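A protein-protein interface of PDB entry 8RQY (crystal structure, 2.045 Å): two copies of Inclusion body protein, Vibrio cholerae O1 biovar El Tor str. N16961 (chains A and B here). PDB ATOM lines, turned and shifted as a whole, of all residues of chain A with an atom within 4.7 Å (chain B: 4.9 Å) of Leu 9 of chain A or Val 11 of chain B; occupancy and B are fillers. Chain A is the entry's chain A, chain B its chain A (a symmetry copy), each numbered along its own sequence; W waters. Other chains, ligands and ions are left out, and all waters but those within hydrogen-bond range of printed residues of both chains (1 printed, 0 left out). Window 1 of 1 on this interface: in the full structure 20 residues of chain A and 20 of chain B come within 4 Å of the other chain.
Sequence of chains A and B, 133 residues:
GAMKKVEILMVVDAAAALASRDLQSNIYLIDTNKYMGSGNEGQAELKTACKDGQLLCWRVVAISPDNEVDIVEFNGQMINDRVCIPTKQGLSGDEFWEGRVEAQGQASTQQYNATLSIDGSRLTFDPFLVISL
Leu 9 of chain A touches just one residue of chain B: Val 11 (3.5 Å).
Of chain A, only Leu 9 comes within 4 Å of Val 11 of chain B.
Printed residues of chain B within 4 Å of Val 11 of chain A: Leu 9 (3.5 Å).
Printed residues of chain B within 4 Å of Glu 7 of chain A: Ile 63 (3.4 Å).
Of the printed residues of chain A, Ala 62 of chain B touches Arg 59.
Printed residues of chain A within 4 Å of Val 61 of chain B: Arg 59.
Leu 29 of chain A touches none of the printed residues of chain B.
The nearest printed residue of chain A that does not touch Tyr 28 of chain B is Leu 29 of chain A (7.1 Å).
N of Arg 59 of chain A lies within hydrogen-bond range of O of Ile 8 of chain A, at 3.1 Å.
N of Leu 9 of chain A is in hydrogen-bond range of O of Ile 30 of chain A (2.8 Å).
N of Met 10 of chain A sits at hydrogen-bond distance from O of Arg 59 of chain A, 2.9 Å away.
The backbone NH (N) of Val 11 of chain A lies within hydrogen-bond range of the backbone carbonyl oxygen (O) of Tyr 28 of chain A.
The backbone carbonyl oxygen (O) of Met 10 of chain B is in hydrogen-bond range of the backbone NH (N) of Val 61 of chain B (2.9 Å).
The backbone NH (N) of Val 12 of chain B is in hydrogen-bond range of the backbone carbonyl oxygen (O) of Val 61 of chain B, at 2.9 Å.
The backbone carbonyl oxygen of Ala 62 of chain B is in hydrogen-bond range of the guanidinium group of Arg 59 of chain A (2.7 Å).
The backbone carbonyl oxygen of Ile 63 of chain B is in hydrogen-bond range of the guanidinium group of Arg 59 of chain A, at 3.2 Å.
Water W1 lies within hydrogen-bond range of the backbone carbonyl oxygen of Ile 63 of chain B and the backbone carbonyl oxygen of Ile 8 of chain A.
Leu 9 of chain A touches Val 11 of chain B, and with the chains exchanged Val 11 of chain A touches Leu 9 of chain B.
Among the printed residues, pairs that only touch across the chains: Glu 7 of chain A with Ile 63 of chain B (3.4 Å), Leu 9 of chain A with Val 11 of chain B (3.5 Å), Val 11 of chain A with Leu 9 of chain B (3.5 Å), Ile 30 of chain A with Tyr 28 of chain B (3.6 Å), Ile 30 of chain A with Ile 63 of chain B (3.7 Å) and Arg 59 of chain A with Val 61 of chain B (3.7 Å).
Of the 10 printed residues of chain A, 5 touch a printed residue of chain B.
Hydrophobic or aromatic side chains of chain A within 4 Å of the printed part of chain B: Leu 9, Val 11 and Ile 30.
Of the 11 printed residues of chain B, 6 touch a printed residue of chain A.
Hydrophobic or aromatic side chains of chain B that line the printed part of chain A: Leu 9, Val 11, Tyr 28, Val 61 and Ile 63.
Along chain B the printed residues that touch a printed residue of chain A span positions 9 to 63.
Among the printed residues, 8 pairs touch across the chains.
Among the printed residues, no Asp or Glu carboxylate lies within 4 Å of a Lys or Arg side-chain nitrogen of the other chain.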
ATOM      1  N   GLU A   7     -21.299  18.363  -5.561  1.00  0.00           N
ATOM      2  CA  GLU A   7     -21.581  19.593  -4.856  1.00  0.00           C
ATOM      3  C   GLU A   7     -21.430  20.774  -5.788  1.00  0.00           C
ATOM      4  O   GLU A   7     -20.444  20.909  -6.516  1.00  0.00           O
ATOM      5  CB  GLU A   7     -20.675  19.621  -3.656  1.00  0.00           C
ATOM      6  CG  GLU A   7     -21.092  18.556  -2.646  1.00  0.00           C
ATOM      7  CD  GLU A   7     -20.045  18.264  -1.579  1.00  0.00           C
ATOM      8  OE1 GLU A   7     -18.930  17.813  -1.956  1.00  0.00           O
ATOM      9  OE2 GLU A   7     -20.310  18.541  -0.379  1.00  0.00           O
ATOM     10  N   ILE A   8     -22.465  21.607  -5.759  1.00  0.00           N
ATOM     11  CA  ILE A   8     -22.669  22.710  -6.671  1.00  0.00           C
ATOM     12  C   ILE A   8     -22.691  23.986  -5.827  1.00  0.00           C
ATOM     13  O   ILE A   8     -23.416  24.068  -4.836  1.00  0.00           O
ATOM     14  CB  ILE A   8     -23.996  22.521  -7.441  1.00  0.00           C
ATOM     15  CG1 ILE A   8     -24.191  21.089  -7.959  1.00  0.00           C
ATOM     16  CG2 ILE A   8     -24.108  23.548  -8.566  1.00  0.00           C
ATOM     17  CD1 ILE A   8     -25.590  20.689  -8.287  1.00  0.00           C
ATOM     18  N   LEU A   9     -21.913  24.998  -6.217  1.00  0.00           N
ATOM     19  CA  LEU A   9     -21.949  26.321  -5.621  1.00  0.00           C
ATOM     20  C   LEU A   9     -22.476  27.290  -6.676  1.00  0.00           C
ATOM     21  O   LEU A   9     -21.929  27.405  -7.776  1.00  0.00           O
ATOM     22  CB  LEU A   9     -20.526  26.727  -5.256  1.00  0.00           C
ATOM     23  CG  LEU A   9     -20.378  28.101  -4.596  1.00  0.00           C
ATOM     24  CD1 LEU A   9     -21.063  28.047  -3.262  1.00  0.00           C
ATOM     25  CD2 LEU A   9     -18.905  28.464  -4.431  1.00  0.00           C
ATOM     26  N   MET A  10     -23.592  27.930  -6.390  1.00  0.00           N
ATOM     27  CA  MET A  10     -24.070  29.051  -7.179  1.00  0.00           C
ATOM     28  C   MET A  10     -23.425  30.305  -6.577  1.00  0.00           C
ATOM     29  O   MET A  10     -23.474  30.521  -5.346  1.00  0.00           O
ATOM     30  CB  MET A  10     -25.593  29.184  -7.037  1.00  0.00           C
ATOM     31  CG  MET A  10     -26.457  28.086  -7.691  1.00  0.00           C
ATOM     32  SD  MET A  10     -28.229  28.242  -7.196  1.00  0.00           S
ATOM     33  CE  MET A  10     -28.838  26.647  -7.671  1.00  0.00           C
ATOM     34  N   VAL A  11     -22.804  31.110  -7.436  1.00  0.00           N
ATOM     35  CA  VAL A  11     -22.229  32.378  -7.045  1.00  0.00           C
ATOM     36  C   VAL A  11     -23.009  33.506  -7.719  1.00  0.00           C
ATOM     37  O   VAL A  11     -23.085  33.548  -8.938  1.00  0.00           O
ATOM     38  CB  VAL A  11     -20.714  32.475  -7.336  1.00  0.00           C
ATOM     39  CG1 VAL A  11     -20.210  33.861  -6.965  1.00  0.00           C
ATOM     40  CG2 VAL A  11     -19.908  31.385  -6.619  1.00  0.00           C
ATOM     41  N   TYR A  28     -22.884  32.413 -11.550  1.00  0.00           N
ATOM     42  CA  TYR A  28     -21.901  31.414 -11.948  1.00  0.00           C
ATOM     43  C   TYR A  28     -22.216  30.119 -11.214  1.00  0.00           C
ATOM     44  O   TYR A  28     -22.772  30.190 -10.106  1.00  0.00           O
ATOM     45  CB  TYR A  28     -20.506  31.900 -11.572  1.00  0.00           C
ATOM     46  CG  TYR A  28     -20.193  33.311 -12.037  1.00  0.00           C
ATOM     47  CD1 TYR A  28     -20.616  34.408 -11.322  1.00  0.00           C
ATOM     48  CD2 TYR A  28     -19.420  33.556 -13.169  1.00  0.00           C
ATOM     49  CE1 TYR A  28     -20.322  35.705 -11.733  1.00  0.00           C
ATOM     50  CE2 TYR A  28     -19.088  34.845 -13.568  1.00  0.00           C
ATOM     51  CZ  TYR A  28     -19.549  35.923 -12.850  1.00  0.00           C
ATOM     52  OH  TYR A  28     -19.234  37.191 -13.195  1.00  0.00           O
ATOM     53  N   LEU A  29     -21.883  28.975 -11.839  1.00  0.00           N
ATOM     54  CA  LEU A  29     -21.906  27.656 -11.204  1.00  0.00           C
ATOM     55  C   LEU A  29     -20.494  27.085 -11.184  1.00  0.00           C
ATOM     56  O   LEU A  29     -19.809  27.131 -12.206  1.00  0.00           O
ATOM     57  CB  LEU A  29     -22.798  26.685 -11.986  1.00  0.00           C
ATOM     58  CG  LEU A  29     -24.280  27.053 -12.187  1.00  0.00           C
ATOM     59  CD1 LEU A  29     -25.043  25.872 -12.805  1.00  0.00           C
ATOM     60  CD2 LEU A  29     -24.980  27.456 -10.913  1.00  0.00           C
ATOM     61  N   ILE A  30     -20.065  26.552 -10.027  1.00  0.00           N
ATOM     62  CA  ILE A  30     -18.845  25.755  -9.886  1.00  0.00           C
ATOM     63  C   ILE A  30     -19.227  24.514  -9.098  1.00  0.00           C
ATOM     64  O   ILE A  30     -19.906  24.629  -8.094  1.00  0.00           O
ATOM     65  CB  ILE A  30     -17.745  26.555  -9.160  1.00  0.00           C
ATOM     66  CG1 ILE A  30     -17.491  27.906  -9.848  1.00  0.00           C
ATOM     67  CG2 ILE A  30     -16.490  25.710  -9.011  1.00  0.00           C
ATOM     68  CD1 ILE A  30     -16.456  28.823  -9.215  1.00  0.00           C
ATOM     69  N   ARG A  59     -25.688  24.867  -2.829  1.00  0.00           N
ATOM     70  CA  ARG A  59     -25.698  26.032  -1.928  1.00  0.00           C
ATOM     71  C   ARG A  59     -25.357  27.304  -2.736  1.00  0.00           C
ATOM     72  O   ARG A  59     -24.815  27.221  -3.819  1.00  0.00           O
ATOM     73  CB  ARG A  59     -24.826  25.770  -0.693  1.00  0.00           C
ATOM     74  CG  ARG A  59     -23.333  25.919  -0.933  1.00  0.00           C
ATOM     75  CD  ARG A  59     -22.474  25.439   0.215  1.00  0.00           C
ATOM     76  NE  ARG A  59     -21.205  26.158   0.214  1.00  0.00           N
ATOM     77  CZ  ARG A  59     -20.972  27.347   0.775  1.00  0.00           C
ATOM     78  NH1 ARG A  59     -21.823  27.848   1.628  1.00  0.00           N
ATOM     79  NH2 ARG A  59     -19.836  28.000   0.583  1.00  0.00           N
ATOM     80  N   VAL A  61     -23.989  31.566  -2.642  1.00  0.00           N
ATOM     81  CA  VAL A  61     -23.247  32.614  -1.934  1.00  0.00           C
ATOM     82  C   VAL A  61     -23.182  33.835  -2.849  1.00  0.00           C
ATOM     83  O   VAL A  61     -23.362  33.736  -4.090  1.00  0.00           O
ATOM     84  CB  VAL A  61     -21.837  32.195  -1.456  1.00  0.00           C
ATOM     85  CG1 VAL A  61     -21.830  31.049  -0.478  1.00  0.00           C
ATOM     86  CG2 VAL A  61     -20.920  31.857  -2.598  1.00  0.00           C
ATOM     87  N   LEU B   9     -14.157  36.996  -4.752  1.00  0.00           N
ATOM     88  CA  LEU B   9     -14.506  35.764  -4.067  1.00  0.00           C
ATOM     89  C   LEU B   9     -13.526  34.688  -4.525  1.00  0.00           C
ATOM     90  O   LEU B   9     -13.386  34.409  -5.719  1.00  0.00           O
ATOM     91  CB  LEU B   9     -15.911  35.354  -4.490  1.00  0.00           C
ATOM     92  CG  LEU B   9     -16.449  34.074  -3.846  1.00  0.00           C
ATOM     93  CD1 LEU B   9     -16.604  34.328  -2.376  1.00  0.00           C
ATOM     94  CD2 LEU B   9     -17.785  33.678  -4.468  1.00  0.00           C
ATOM     95  N   MET B  10     -12.774  34.134  -3.595  1.00  0.00           N
ATOM     96  CA  MET B  10     -11.986  32.939  -3.840  1.00  0.00           C
ATOM     97  C   MET B  10     -12.904  31.751  -3.531  1.00  0.00           C
ATOM     98  O   MET B  10     -13.544  31.699  -2.458  1.00  0.00           O
ATOM     99  CB  MET B  10     -10.795  32.886  -2.872  1.00  0.00           C
ATOM    100  CG  MET B  10      -9.672  33.921  -3.084  1.00  0.00           C
ATOM    101  SD  MET B  10      -8.468  33.901  -1.685  1.00  0.00           S
ATOM    102  CE  MET B  10      -7.635  35.443  -1.953  1.00  0.00           C
ATOM    103  N   VAL B  11     -12.985  30.817  -4.476  1.00  0.00           N
ATOM    104  CA  VAL B  11     -13.729  29.590  -4.301  1.00  0.00           C
ATOM    105  C   VAL B  11     -12.753  28.414  -4.285  1.00  0.00           C
ATOM    106  O   VAL B  11     -12.023  28.216  -5.247  1.00  0.00           O
ATOM    107  CB  VAL B  11     -14.841  29.396  -5.358  1.00  0.00           C
ATOM    108  CG1 VAL B  11     -15.519  28.051  -5.146  1.00  0.00           C
ATOM    109  CG2 VAL B  11     -15.864  30.538  -5.348  1.00  0.00           C
ATOM    110  N   VAL B  12     -12.796  27.628  -3.189  1.00  0.00           N
ATOM    111  CA  VAL B  12     -11.953  26.462  -3.023  1.00  0.00           C
ATOM    112  C   VAL B  12     -12.760  25.152  -3.155  1.00  0.00           C
ATOM    113  O   VAL B  12     -13.790  24.951  -2.521  1.00  0.00           O
ATOM    114  CB  VAL B  12     -11.258  26.510  -1.666  1.00  0.00           C
ATOM    115  CG1 VAL B  12     -10.216  25.390  -1.588  1.00  0.00           C
ATOM    116  CG2 VAL B  12     -10.636  27.861  -1.377  1.00  0.00           C
ATOM    117  N   ASP B  13     -12.293  24.252  -4.035  1.00  0.00           N
ATOM    118  CA  ASP B  13     -12.669  22.832  -4.026  1.00  0.00           C
ATOM    119  C   ASP B  13     -11.867  22.164  -2.893  1.00  0.00           C
ATOM    120  O   ASP B  13     -10.778  21.693  -3.129  1.00  0.00           O
ATOM    121  CB  ASP B  13     -12.383  22.165  -5.388  1.00  0.00           C
ATOM    122  CG  ASP B  13     -12.948  20.745  -5.538  1.00  0.00           C
ATOM    123  OD1 ASP B  13     -13.282  20.100  -4.443  1.00  0.00           O
ATOM    124  OD2 ASP B  13     -13.075  20.266  -6.788  1.00  0.00           O
ATOM    125  N   ASN B  26      -6.961  23.975  -7.522  1.00  0.00           N
ATOM    126  CA  ASN B  26      -8.272  23.735  -6.996  1.00  0.00           C
ATOM    127  C   ASN B  26      -8.927  25.013  -6.502  1.00  0.00           C
ATOM    128  O   ASN B  26      -9.759  24.939  -5.592  1.00  0.00           O
ATOM    129  CB  ASN B  26      -8.077  22.724  -5.883  1.00  0.00           C
ATOM    130  CG  ASN B  26      -7.766  21.368  -6.463  1.00  0.00           C
ATOM    131  OD1 ASN B  26      -8.599  20.834  -7.177  1.00  0.00           O
ATOM    132  ND2 ASN B  26      -6.608  20.818  -6.148  1.00  0.00           N
ATOM    133  N   ILE B  27      -8.575  26.171  -7.092  1.00  0.00           N
ATOM    134  CA  ILE B  27      -9.145  27.426  -6.651  1.00  0.00           C
ATOM    135  C   ILE B  27      -9.673  28.180  -7.882  1.00  0.00           C
ATOM    136  O   ILE B  27      -9.210  27.967  -8.986  1.00  0.00           O
ATOM    137  CB  ILE B  27      -8.128  28.233  -5.816  1.00  0.00           C
ATOM    138  CG1 ILE B  27      -8.812  29.216  -4.871  1.00  0.00           C
ATOM    139  CG2 ILE B  27      -7.105  28.900  -6.713  1.00  0.00           C
ATOM    140  CD1 ILE B  27      -7.937  29.612  -3.737  1.00  0.00           C
ATOM    141  N   TYR B  28     -10.719  28.993  -7.664  1.00  0.00           N
ATOM    142  CA  TYR B  28     -11.285  29.892  -8.662  1.00  0.00           C
ATOM    143  C   TYR B  28     -11.371  31.283  -8.051  1.00  0.00           C
ATOM    144  O   TYR B  28     -11.515  31.379  -6.822  1.00  0.00           O
ATOM    145  CB  TYR B  28     -12.676  29.405  -9.051  1.00  0.00           C
ATOM    146  CG  TYR B  28     -12.738  27.934  -9.422  1.00  0.00           C
ATOM    147  CD1 TYR B  28     -12.819  26.957  -8.456  1.00  0.00           C
ATOM    148  CD2 TYR B  28     -12.775  27.513 -10.749  1.00  0.00           C
ATOM    149  CE1 TYR B  28     -12.891  25.607  -8.787  1.00  0.00           C
ATOM    150  CE2 TYR B  28     -12.885  26.171 -11.092  1.00  0.00           C
ATOM    151  CZ  TYR B  28     -12.934  25.216 -10.105  1.00  0.00           C
ATOM    152  OH  TYR B  28     -13.058  23.902 -10.398  1.00  0.00           O
ATOM    153  N   VAL B  61     -14.633  31.037   0.196  1.00  0.00           N
ATOM    154  CA  VAL B  61     -15.682  30.062   0.512  1.00  0.00           C
ATOM    155  C   VAL B  61     -15.283  28.730  -0.121  1.00  0.00           C
ATOM    156  O   VAL B  61     -14.451  28.673  -1.061  1.00  0.00           O
ATOM    157  CB  VAL B  61     -17.107  30.484   0.082  1.00  0.00           C
ATOM    158  CG1 VAL B  61     -17.602  31.746   0.738  1.00  0.00           C
ATOM    159  CG2 VAL B  61     -17.235  30.634  -1.408  1.00  0.00           C
ATOM    160  N   ALA B  62     -15.822  27.650   0.473  1.00  0.00           N
ATOM    161  CA  ALA B  62     -15.676  26.298  -0.061  1.00  0.00           C
ATOM    162  C   ALA B  62     -16.933  25.896  -0.855  1.00  0.00           C
ATOM    163  O   ALA B  62     -18.029  26.388  -0.573  1.00  0.00           O
ATOM    164  CB  ALA B  62     -15.382  25.308   1.026  1.00  0.00           C
ATOM    165  N   ILE B  63     -16.767  25.007  -1.862  1.00  0.00           N
ATOM    166  CA  ILE B  63     -17.909  24.538  -2.654  1.00  0.00           C
ATOM    167  C   ILE B  63     -18.818  23.714  -1.749  1.00  0.00           C
ATOM    168  O   ILE B  63     -20.036  23.902  -1.734  1.00  0.00           O
ATOM    169  CB  ILE B  63     -17.467  23.721  -3.883  1.00  0.00           C
ATOM    170  CG1 ILE B  63     -16.620  24.553  -4.854  1.00  0.00           C
ATOM    171  CG2 ILE B  63     -18.689  23.074  -4.550  1.00  0.00           C
ATOM    172  CD1 ILE B  63     -15.943  23.742  -5.958  1.00  0.00           C
HETATM  173  O   HOH W   1     -22.517  22.769  -2.238  1.00  0.00           O
